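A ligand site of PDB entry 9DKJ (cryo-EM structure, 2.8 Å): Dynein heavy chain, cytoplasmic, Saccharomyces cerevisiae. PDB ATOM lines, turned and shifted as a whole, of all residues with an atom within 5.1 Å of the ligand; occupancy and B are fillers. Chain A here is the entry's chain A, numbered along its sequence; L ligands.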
ATOM      1  N   VAL A1513     -31.628 -36.804  10.775  1.00  0.00           N
ATOM      2  CA  VAL A1513     -30.848 -35.785  11.470  1.00  0.00           C
ATOM      3  C   VAL A1513     -30.779 -36.169  12.942  1.00  0.00           C
ATOM      4  O   VAL A1513     -31.721 -35.892  13.697  1.00  0.00           O
ATOM      5  CB  VAL A1513     -31.450 -34.380  11.282  1.00  0.00           C
ATOM      6  CG1 VAL A1513     -30.561 -33.335  11.945  1.00  0.00           C
ATOM      7  CG2 VAL A1513     -31.632 -34.069   9.816  1.00  0.00           C
ATOM      8  N   PRO A1514     -29.700 -36.800  13.402  1.00  0.00           N
ATOM      9  CA  PRO A1514     -29.640 -37.312  14.787  1.00  0.00           C
ATOM     10  C   PRO A1514     -29.411 -36.231  15.833  1.00  0.00           C
ATOM     11  O   PRO A1514     -28.295 -35.939  16.264  1.00  0.00           O
ATOM     12  CB  PRO A1514     -28.472 -38.298  14.725  1.00  0.00           C
ATOM     13  CG  PRO A1514     -27.593 -37.774  13.644  1.00  0.00           C
ATOM     14  CD  PRO A1514     -28.491 -37.137  12.622  1.00  0.00           C
ATOM     15  N   MET A1515     -30.505 -35.604  16.275  1.00  0.00           N
ATOM     16  CA  MET A1515     -30.419 -34.586  17.309  1.00  0.00           C
ATOM     17  C   MET A1515     -30.816 -35.167  18.660  1.00  0.00           C
ATOM     18  O   MET A1515     -31.049 -36.368  18.812  1.00  0.00           O
ATOM     19  CB  MET A1515     -31.287 -33.378  16.983  1.00  0.00           C
ATOM     20  CG  MET A1515     -30.866 -32.602  15.752  1.00  0.00           C
ATOM     21  SD  MET A1515     -31.917 -31.156  15.581  1.00  0.00           S
ATOM     22  CE  MET A1515     -33.419 -31.952  15.087  1.00  0.00           C
ATOM     23  N   VAL A1516     -30.888 -34.288  19.655  1.00  0.00           N
ATOM     24  CA  VAL A1516     -31.185 -34.669  21.024  1.00  0.00           C
ATOM     25  C   VAL A1516     -32.304 -33.762  21.532  1.00  0.00           C
ATOM     26  O   VAL A1516     -32.536 -32.675  21.003  1.00  0.00           O
ATOM     27  CB  VAL A1516     -29.924 -34.589  21.914  1.00  0.00           C
ATOM     28  CG1 VAL A1516     -29.575 -33.154  22.251  1.00  0.00           C
ATOM     29  CG2 VAL A1516     -30.047 -35.465  23.151  1.00  0.00           C
ATOM     30  N   HIS A1518     -34.582 -31.504  24.124  1.00  0.00           N
ATOM     31  CA  HIS A1518     -34.516 -30.584  25.244  1.00  0.00           C
ATOM     32  C   HIS A1518     -35.751 -29.699  25.265  1.00  0.00           C
ATOM     33  O   HIS A1518     -36.498 -29.597  24.280  1.00  0.00           O
ATOM     34  CB  HIS A1518     -33.220 -29.746  25.205  1.00  0.00           C
ATOM     35  CG  HIS A1518     -32.968 -29.069  23.889  1.00  0.00           C
ATOM     36  ND1 HIS A1518     -33.317 -27.764  23.646  1.00  0.00           N
ATOM     37  CD2 HIS A1518     -32.394 -29.527  22.754  1.00  0.00           C
ATOM     38  CE1 HIS A1518     -32.965 -27.438  22.412  1.00  0.00           C
ATOM     39  NE2 HIS A1518     -32.407 -28.500  21.848  1.00  0.00           N
ATOM     40  N   MET A1521     -36.434 -26.807  22.648  1.00  0.00           N
ATOM     41  CA  MET A1521     -36.901 -27.268  21.342  1.00  0.00           C
ATOM     42  C   MET A1521     -38.321 -27.831  21.473  1.00  0.00           C
ATOM     43  O   MET A1521     -39.124 -27.689  20.549  1.00  0.00           O
ATOM     44  CB  MET A1521     -35.942 -28.312  20.767  1.00  0.00           C
ATOM     45  CG  MET A1521     -36.536 -29.129  19.631  1.00  0.00           C
ATOM     46  SD  MET A1521     -35.770 -30.680  19.218  1.00  0.00           S
ATOM     47  CE  MET A1521     -35.962 -31.443  20.787  1.00  0.00           C
ATOM     48  N   ALA A1544     -30.343 -18.095  15.850  1.00  0.00           N
ATOM     49  CA  ALA A1544     -28.993 -18.282  15.352  1.00  0.00           C
ATOM     50  C   ALA A1544     -28.932 -19.461  14.377  1.00  0.00           C
ATOM     51  O   ALA A1544     -29.852 -20.286  14.307  1.00  0.00           O
ATOM     52  CB  ALA A1544     -28.012 -18.499  16.496  1.00  0.00           C
ATOM     53  N   SER A1545     -27.851 -19.532  13.631  1.00  0.00           N
ATOM     54  CA  SER A1545     -27.675 -20.617  12.672  1.00  0.00           C
ATOM     55  C   SER A1545     -27.422 -21.934  13.409  1.00  0.00           C
ATOM     56  O   SER A1545     -26.836 -21.957  14.487  1.00  0.00           O
ATOM     57  CB  SER A1545     -26.529 -20.320  11.710  1.00  0.00           C
ATOM     58  OG  SER A1545     -26.451 -21.312  10.706  1.00  0.00           O
ATOM     59  N   ARG A1546     -27.889 -23.023  12.800  1.00  0.00           N
ATOM     60  CA  ARG A1546     -27.789 -24.382  13.335  1.00  0.00           C
ATOM     61  C   ARG A1546     -28.446 -24.512  14.705  1.00  0.00           C
ATOM     62  O   ARG A1546     -27.991 -25.252  15.577  1.00  0.00           O
ATOM     63  CB  ARG A1546     -26.333 -24.857  13.392  1.00  0.00           C
ATOM     64  CG  ARG A1546     -25.822 -25.420  12.074  1.00  0.00           C
ATOM     65  CD  ARG A1546     -24.446 -26.028  12.237  1.00  0.00           C
ATOM     66  NE  ARG A1546     -24.511 -27.408  12.687  1.00  0.00           N
ATOM     67  CZ  ARG A1546     -23.484 -28.100  13.152  1.00  0.00           C
ATOM     68  NH1 ARG A1546     -22.275 -27.566  13.235  1.00  0.00           N
ATOM     69  NH2 ARG A1546     -23.667 -29.351  13.553  1.00  0.00           N
ATOM     70  N   THR A1547     -29.547 -23.774  14.908  1.00  0.00           N
ATOM     71  CA  THR A1547     -30.341 -23.880  16.123  1.00  0.00           C
ATOM     72  C   THR A1547     -31.454 -24.904  15.976  1.00  0.00           C
ATOM     73  O   THR A1547     -31.775 -25.615  16.944  1.00  0.00           O
ATOM     74  CB  THR A1547     -30.916 -22.505  16.499  1.00  0.00           C
ATOM     75  OG1 THR A1547     -29.852 -21.540  16.517  1.00  0.00           O
ATOM     76  CG2 THR A1547     -31.569 -22.536  17.863  1.00  0.00           C
ATOM     77  N   GLY A1548     -32.030 -25.022  14.794  1.00  0.00           N
ATOM     78  CA  GLY A1548     -33.037 -26.037  14.564  1.00  0.00           C
ATOM     79  C   GLY A1548     -34.321 -25.540  13.933  1.00  0.00           C
ATOM     80  O   GLY A1548     -35.322 -26.263  13.953  1.00  0.00           O
ATOM     81  N   LYS A1549     -34.298 -24.328  13.381  1.00  0.00           N
ATOM     82  CA  LYS A1549     -35.522 -23.722  12.862  1.00  0.00           C
ATOM     83  C   LYS A1549     -36.115 -24.523  11.713  1.00  0.00           C
ATOM     84  O   LYS A1549     -37.302 -24.874  11.721  1.00  0.00           O
ATOM     85  CB  LYS A1549     -35.224 -22.288  12.412  1.00  0.00           C
ATOM     86  CG  LYS A1549     -34.670 -21.403  13.506  1.00  0.00           C
ATOM     87  CD  LYS A1549     -34.163 -20.092  12.945  1.00  0.00           C
ATOM     88  CE  LYS A1549     -32.932 -20.296  12.089  1.00  0.00           C
ATOM     89  NZ  LYS A1549     -31.680 -20.005  12.826  1.00  0.00           N
ATOM     90  N   THR A1550     -35.289 -24.846  10.703  1.00  0.00           N
ATOM     91  CA  THR A1550     -35.769 -25.544   9.522  1.00  0.00           C
ATOM     92  C   THR A1550     -36.213 -26.969   9.858  1.00  0.00           C
ATOM     93  O   THR A1550     -37.268 -27.417   9.383  1.00  0.00           O
ATOM     94  CB  THR A1550     -34.683 -25.569   8.445  1.00  0.00           C
ATOM     95  OG1 THR A1550     -34.113 -24.259   8.329  1.00  0.00           O
ATOM     96  CG2 THR A1550     -35.269 -25.974   7.114  1.00  0.00           C
ATOM     97  N   ILE A1551     -35.439 -27.677  10.675  1.00  0.00           N
ATOM     98  CA  ILE A1551     -35.781 -29.056  11.002  1.00  0.00           C
ATOM     99  C   ILE A1551     -37.010 -29.111  11.909  1.00  0.00           C
ATOM    100  O   ILE A1551     -37.806 -30.054  11.809  1.00  0.00           O
ATOM    101  CB  ILE A1551     -34.558 -29.775  11.605  1.00  0.00           C
ATOM    102  CG1 ILE A1551     -34.780 -31.295  11.646  1.00  0.00           C
ATOM    103  CG2 ILE A1551     -34.184 -29.199  12.953  1.00  0.00           C
ATOM    104  CD1 ILE A1551     -34.876 -31.933  10.287  1.00  0.00           C
ATOM    105  N   THR A1673     -37.536 -18.368   7.880  1.00  0.00           N
ATOM    106  CA  THR A1673     -36.370 -18.742   8.654  1.00  0.00           C
ATOM    107  C   THR A1673     -35.310 -17.657   8.489  1.00  0.00           C
ATOM    108  O   THR A1673     -34.885 -17.371   7.362  1.00  0.00           O
ATOM    109  CB  THR A1673     -35.849 -20.102   8.203  1.00  0.00           C
ATOM    110  OG1 THR A1673     -36.752 -21.130   8.635  1.00  0.00           O
ATOM    111  CG2 THR A1673     -34.477 -20.373   8.791  1.00  0.00           C
ATOM    112  N   CYS A1675     -31.595 -16.233  10.020  1.00  0.00           N
ATOM    113  CA  CYS A1675     -30.427 -16.587  10.803  1.00  0.00           C
ATOM    114  C   CYS A1675     -29.753 -15.366  11.427  1.00  0.00           C
ATOM    115  O   CYS A1675     -29.529 -15.326  12.640  1.00  0.00           O
ATOM    116  CB  CYS A1675     -29.421 -17.363   9.942  1.00  0.00           C
ATOM    117  SG  CYS A1675     -29.944 -19.039   9.523  1.00  0.00           S
ATOM    118  N   TRP A1703     -28.874 -20.603  21.741  1.00  0.00           N
ATOM    119  CA  TRP A1703     -28.962 -21.482  22.898  1.00  0.00           C
ATOM    120  C   TRP A1703     -28.438 -20.778  24.149  1.00  0.00           C
ATOM    121  O   TRP A1703     -27.448 -20.045  24.095  1.00  0.00           O
ATOM    122  CB  TRP A1703     -28.166 -22.764  22.660  1.00  0.00           C
ATOM    123  CG  TRP A1703     -28.806 -23.713  21.708  1.00  0.00           C
ATOM    124  CD1 TRP A1703     -29.928 -23.505  20.954  1.00  0.00           C
ATOM    125  CD2 TRP A1703     -28.367 -25.045  21.398  1.00  0.00           C
ATOM    126  NE1 TRP A1703     -30.214 -24.613  20.200  1.00  0.00           N
ATOM    127  CE2 TRP A1703     -29.269 -25.578  20.456  1.00  0.00           C
ATOM    128  CE3 TRP A1703     -27.305 -25.837  21.840  1.00  0.00           C
ATOM    129  CZ2 TRP A1703     -29.138 -26.858  19.945  1.00  0.00           C
ATOM    130  CZ3 TRP A1703     -27.174 -27.117  21.329  1.00  0.00           C
ATOM    131  CH2 TRP A1703     -28.085 -27.608  20.390  1.00  0.00           C
ATOM    132  N   VAL A1711     -28.214 -30.501  26.327  1.00  0.00           N
ATOM    133  CA  VAL A1711     -27.794 -31.187  25.110  1.00  0.00           C
ATOM    134  C   VAL A1711     -26.491 -31.954  25.350  1.00  0.00           C
ATOM    135  O   VAL A1711     -26.379 -33.146  24.989  1.00  0.00           O
ATOM    136  CB  VAL A1711     -27.629 -30.164  23.967  1.00  0.00           C
ATOM    137  CG1 VAL A1711     -26.819 -30.739  22.819  1.00  0.00           C
ATOM    138  CG2 VAL A1711     -28.986 -29.696  23.487  1.00  0.00           C
ATOM    139  N   MET A1715     -25.979 -36.085  25.415  1.00  0.00           N
ATOM    140  CA  MET A1715     -25.230 -36.854  24.424  1.00  0.00           C
ATOM    141  C   MET A1715     -23.768 -37.077  24.792  1.00  0.00           C
ATOM    142  O   MET A1715     -22.953 -37.359  23.907  1.00  0.00           O
ATOM    143  CB  MET A1715     -25.346 -36.238  23.022  1.00  0.00           C
ATOM    144  CG  MET A1715     -24.729 -34.873  22.801  1.00  0.00           C
ATOM    145  SD  MET A1715     -25.058 -34.408  21.085  1.00  0.00           S
ATOM    146  CE  MET A1715     -24.294 -32.796  20.983  1.00  0.00           C
ATOM    147  N   ILE A1776     -21.790 -28.078  19.228  1.00  0.00           N
ATOM    148  CA  ILE A1776     -22.267 -29.404  18.835  1.00  0.00           C
ATOM    149  C   ILE A1776     -21.152 -30.207  18.173  1.00  0.00           C
ATOM    150  O   ILE A1776     -20.966 -31.395  18.476  1.00  0.00           O
ATOM    151  CB  ILE A1776     -23.500 -29.278  17.924  1.00  0.00           C
ATOM    152  CG1 ILE A1776     -24.657 -28.622  18.677  1.00  0.00           C
ATOM    153  CG2 ILE A1776     -23.935 -30.631  17.406  1.00  0.00           C
ATOM    154  CD1 ILE A1776     -25.626 -27.911  17.756  1.00  0.00           C
ATOM    155  N   ARG A1780     -19.636 -33.866  19.462  1.00  0.00           N
ATOM    156  CA  ARG A1780     -19.557 -35.110  18.687  1.00  0.00           C
ATOM    157  C   ARG A1780     -18.113 -35.574  18.496  1.00  0.00           C
ATOM    158  O   ARG A1780     -17.828 -36.773  18.602  1.00  0.00           O
ATOM    159  CB  ARG A1780     -20.252 -34.969  17.332  1.00  0.00           C
ATOM    160  CG  ARG A1780     -21.582 -34.229  17.368  1.00  0.00           C
ATOM    161  CD  ARG A1780     -22.263 -34.223  16.010  1.00  0.00           C
ATOM    162  NE  ARG A1780     -23.704 -34.058  16.113  1.00  0.00           N
ATOM    163  CZ  ARG A1780     -24.467 -33.471  15.201  1.00  0.00           C
ATOM    164  NH1 ARG A1780     -23.941 -32.971  14.093  1.00  0.00           N
ATOM    165  NH2 ARG A1780     -25.776 -33.377  15.406  1.00  0.00           N
ATOM    166  N   SER A2250     -24.831 -29.900   4.555  1.00  0.00           N
ATOM    167  CA  SER A2250     -25.421 -30.247   5.841  1.00  0.00           C
ATOM    168  C   SER A2250     -25.430 -31.744   6.108  1.00  0.00           C
ATOM    169  O   SER A2250     -25.811 -32.144   7.224  1.00  0.00           O
ATOM    170  CB  SER A2250     -26.847 -29.699   5.931  1.00  0.00           C
ATOM    171  OG  SER A2250     -27.602 -30.053   4.782  1.00  0.00           O
ATOM    172  N   GLU A2252     -27.395 -34.044   5.057  1.00  0.00           N
ATOM    173  CA  GLU A2252     -28.762 -34.470   5.317  1.00  0.00           C
ATOM    174  C   GLU A2252     -29.180 -35.409   4.191  1.00  0.00           C
ATOM    175  O   GLU A2252     -29.528 -34.969   3.092  1.00  0.00           O
ATOM    176  CB  GLU A2252     -29.698 -33.263   5.420  1.00  0.00           C
ATOM    177  CG  GLU A2252     -29.420 -32.380   6.619  1.00  0.00           C
ATOM    178  CD  GLU A2252     -30.309 -31.164   6.657  1.00  0.00           C
ATOM    179  OE1 GLU A2252     -31.041 -30.928   5.673  1.00  0.00           O
ATOM    180  OE2 GLU A2252     -30.276 -30.426   7.671  1.00  0.00           O
ATOM    181  N   ARG A2295     -21.498 -24.584   8.921  1.00  0.00           N
ATOM    182  CA  ARG A2295     -21.469 -26.025   8.715  1.00  0.00           C
ATOM    183  C   ARG A2295     -20.169 -26.558   8.122  1.00  0.00           C
ATOM    184  O   ARG A2295     -20.036 -27.784   8.012  1.00  0.00           O
ATOM    185  CB  ARG A2295     -22.636 -26.442   7.801  1.00  0.00           C
ATOM    186  CG  ARG A2295     -23.998 -26.213   8.410  1.00  0.00           C
ATOM    187  CD  ARG A2295     -25.104 -26.528   7.430  1.00  0.00           C
ATOM    188  NE  ARG A2295     -26.357 -26.868   8.095  1.00  0.00           N
ATOM    189  CZ  ARG A2295     -27.195 -25.997   8.622  1.00  0.00           C
ATOM    190  NH1 ARG A2295     -26.952 -24.700   8.598  1.00  0.00           N
ATOM    191  NH2 ARG A2295     -28.317 -26.437   9.202  1.00  0.00           N
HETATM  192  P1  LIG L   1     -30.770 -24.175  10.724  1.00  0.00           P
HETATM  193  O1  LIG L   1     -29.292 -24.207  10.438  1.00  0.00           O
HETATM  194  O2  LIG L   1     -31.491 -22.976  10.142  1.00  0.00           O
HETATM  195  O3  LIG L   1     -31.150 -24.471  12.147  1.00  0.00           O
HETATM  196  P2  LIG L   1     -31.385 -26.939  10.375  1.00  0.00           P
HETATM  197  O4  LIG L   1     -31.613 -27.824   9.174  1.00  0.00           O
HETATM  198  O5  LIG L   1     -32.340 -27.011  11.537  1.00  0.00           O
HETATM  199  O6  LIG L   1     -31.336 -25.411   9.867  1.00  0.00           O
HETATM  200  O7  LIG L   1     -29.926 -27.283  10.953  1.00  0.00           O
HETATM  201  C1  LIG L   1     -29.739 -27.398  12.355  1.00  0.00           C
HETATM  202  C2  LIG L   1     -28.398 -28.065  12.665  1.00  0.00           C
HETATM  203  O8  LIG L   1     -28.027 -27.780  14.011  1.00  0.00           O
HETATM  204  C3  LIG L   1     -28.480 -29.575  12.501  1.00  0.00           C
HETATM  205  O9  LIG L   1     -27.589 -29.999  11.467  1.00  0.00           O
HETATM  206  C4  LIG L   1     -28.036 -30.151  13.827  1.00  0.00           C
HETATM  207  O10 LIG L   1     -26.845 -30.923  13.646  1.00  0.00           O
HETATM  208  C5  LIG L   1     -27.750 -28.984  14.742  1.00  0.00           C
HETATM  209  N1  LIG L   1     -28.686 -29.042  15.890  1.00  0.00           N
HETATM  210  C6  LIG L   1     -29.668 -28.165  16.148  1.00  0.00           C
HETATM  211  N2  LIG L   1     -30.346 -28.503  17.275  1.00  0.00           N
HETATM  212  C7  LIG L   1     -29.787 -29.630  17.757  1.00  0.00           C
HETATM  213  C8  LIG L   1     -30.026 -30.523  18.913  1.00  0.00           C
HETATM  214  N3  LIG L   1     -31.013 -30.276  19.803  1.00  0.00           N
HETATM  215  N4  LIG L   1     -29.213 -31.593  19.047  1.00  0.00           N
HETATM  216  C9  LIG L   1     -28.226 -31.855  18.169  1.00  0.00           C
HETATM  217  N5  LIG L   1     -27.968 -31.098  17.101  1.00  0.00           N
HETATM  218  C10 LIG L   1     -28.696 -29.980  16.840  1.00  0.00           C
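The guanidinium group (NH2) of Arg 2295 lies within salt-bridge range of an oxygen (O1) of the ligand, at 2.7 Å. The backbone NH (N) of Gly 1548 lies within hydrogen-bond range of an oxygen (O3) of the ligand. The backbone NH of Arg 1546 sits at hydrogen-bond distance from an oxygen (O1) of the ligand, 3.0 Å away. A nitrogen (N3) of the ligand is in hydrogen-bond range of a ring nitrogen (NE2) of His 1518, at 3.0 Å. A nitrogen (N4) of the ligand is in hydrogen-bond range of the backbone NH of Val 1516, at 3.2 Å. The backbone carbonyl oxygen (O) of Val 1516 is in hydrogen-bond range of a nitrogen (N3) of the ligand (3.1 Å). An oxygen (O5) of the ligand sits close to the backbone NH of Ile 1551 (3.3 Å). An oxygen (O10) of the ligand is in hydrogen-bond range of the guanidinium group (NH2) of Arg 1780 (3.2 Å). The backbone NH (N) of Thr 1547 is in hydrogen-bond range of an oxygen (O3) of the ligand, at 3.3 Å. OG1 of Thr 1550 lies within hydrogen-bond range of O6 of the ligand, 3.4 Å away. The backbone NH (N) of Lys 1549 lies within hydrogen-bond range of an oxygen (O3) of the ligand, at 3.4 Å.
N of Met 1521 sits at hydrogen-bond distance from ND1 of His 1518. The side-chain hydroxyl of Thr 1547 is in hydrogen-bond range of the backbone carbonyl oxygen of Ala 1544 (2.5 Å).
The side-chain sulfur of Met 1515 lies close to a nitrogen (N2) of the ligand (3.5 Å). An oxygen (O4) of the ligand sits close to the side-chain carboxylate (OE2) of Glu 2252, 3.3 Å away. Merely in contact with the ligand: Trp 1703 (3.4 Å) and Ile 1776 (3.8 Å). Hydrophobic or aromatic side chains that line the ligand: Met 1515, Val 1516, His 1518, Ile 1551, Trp 1703 and Ile 1776.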
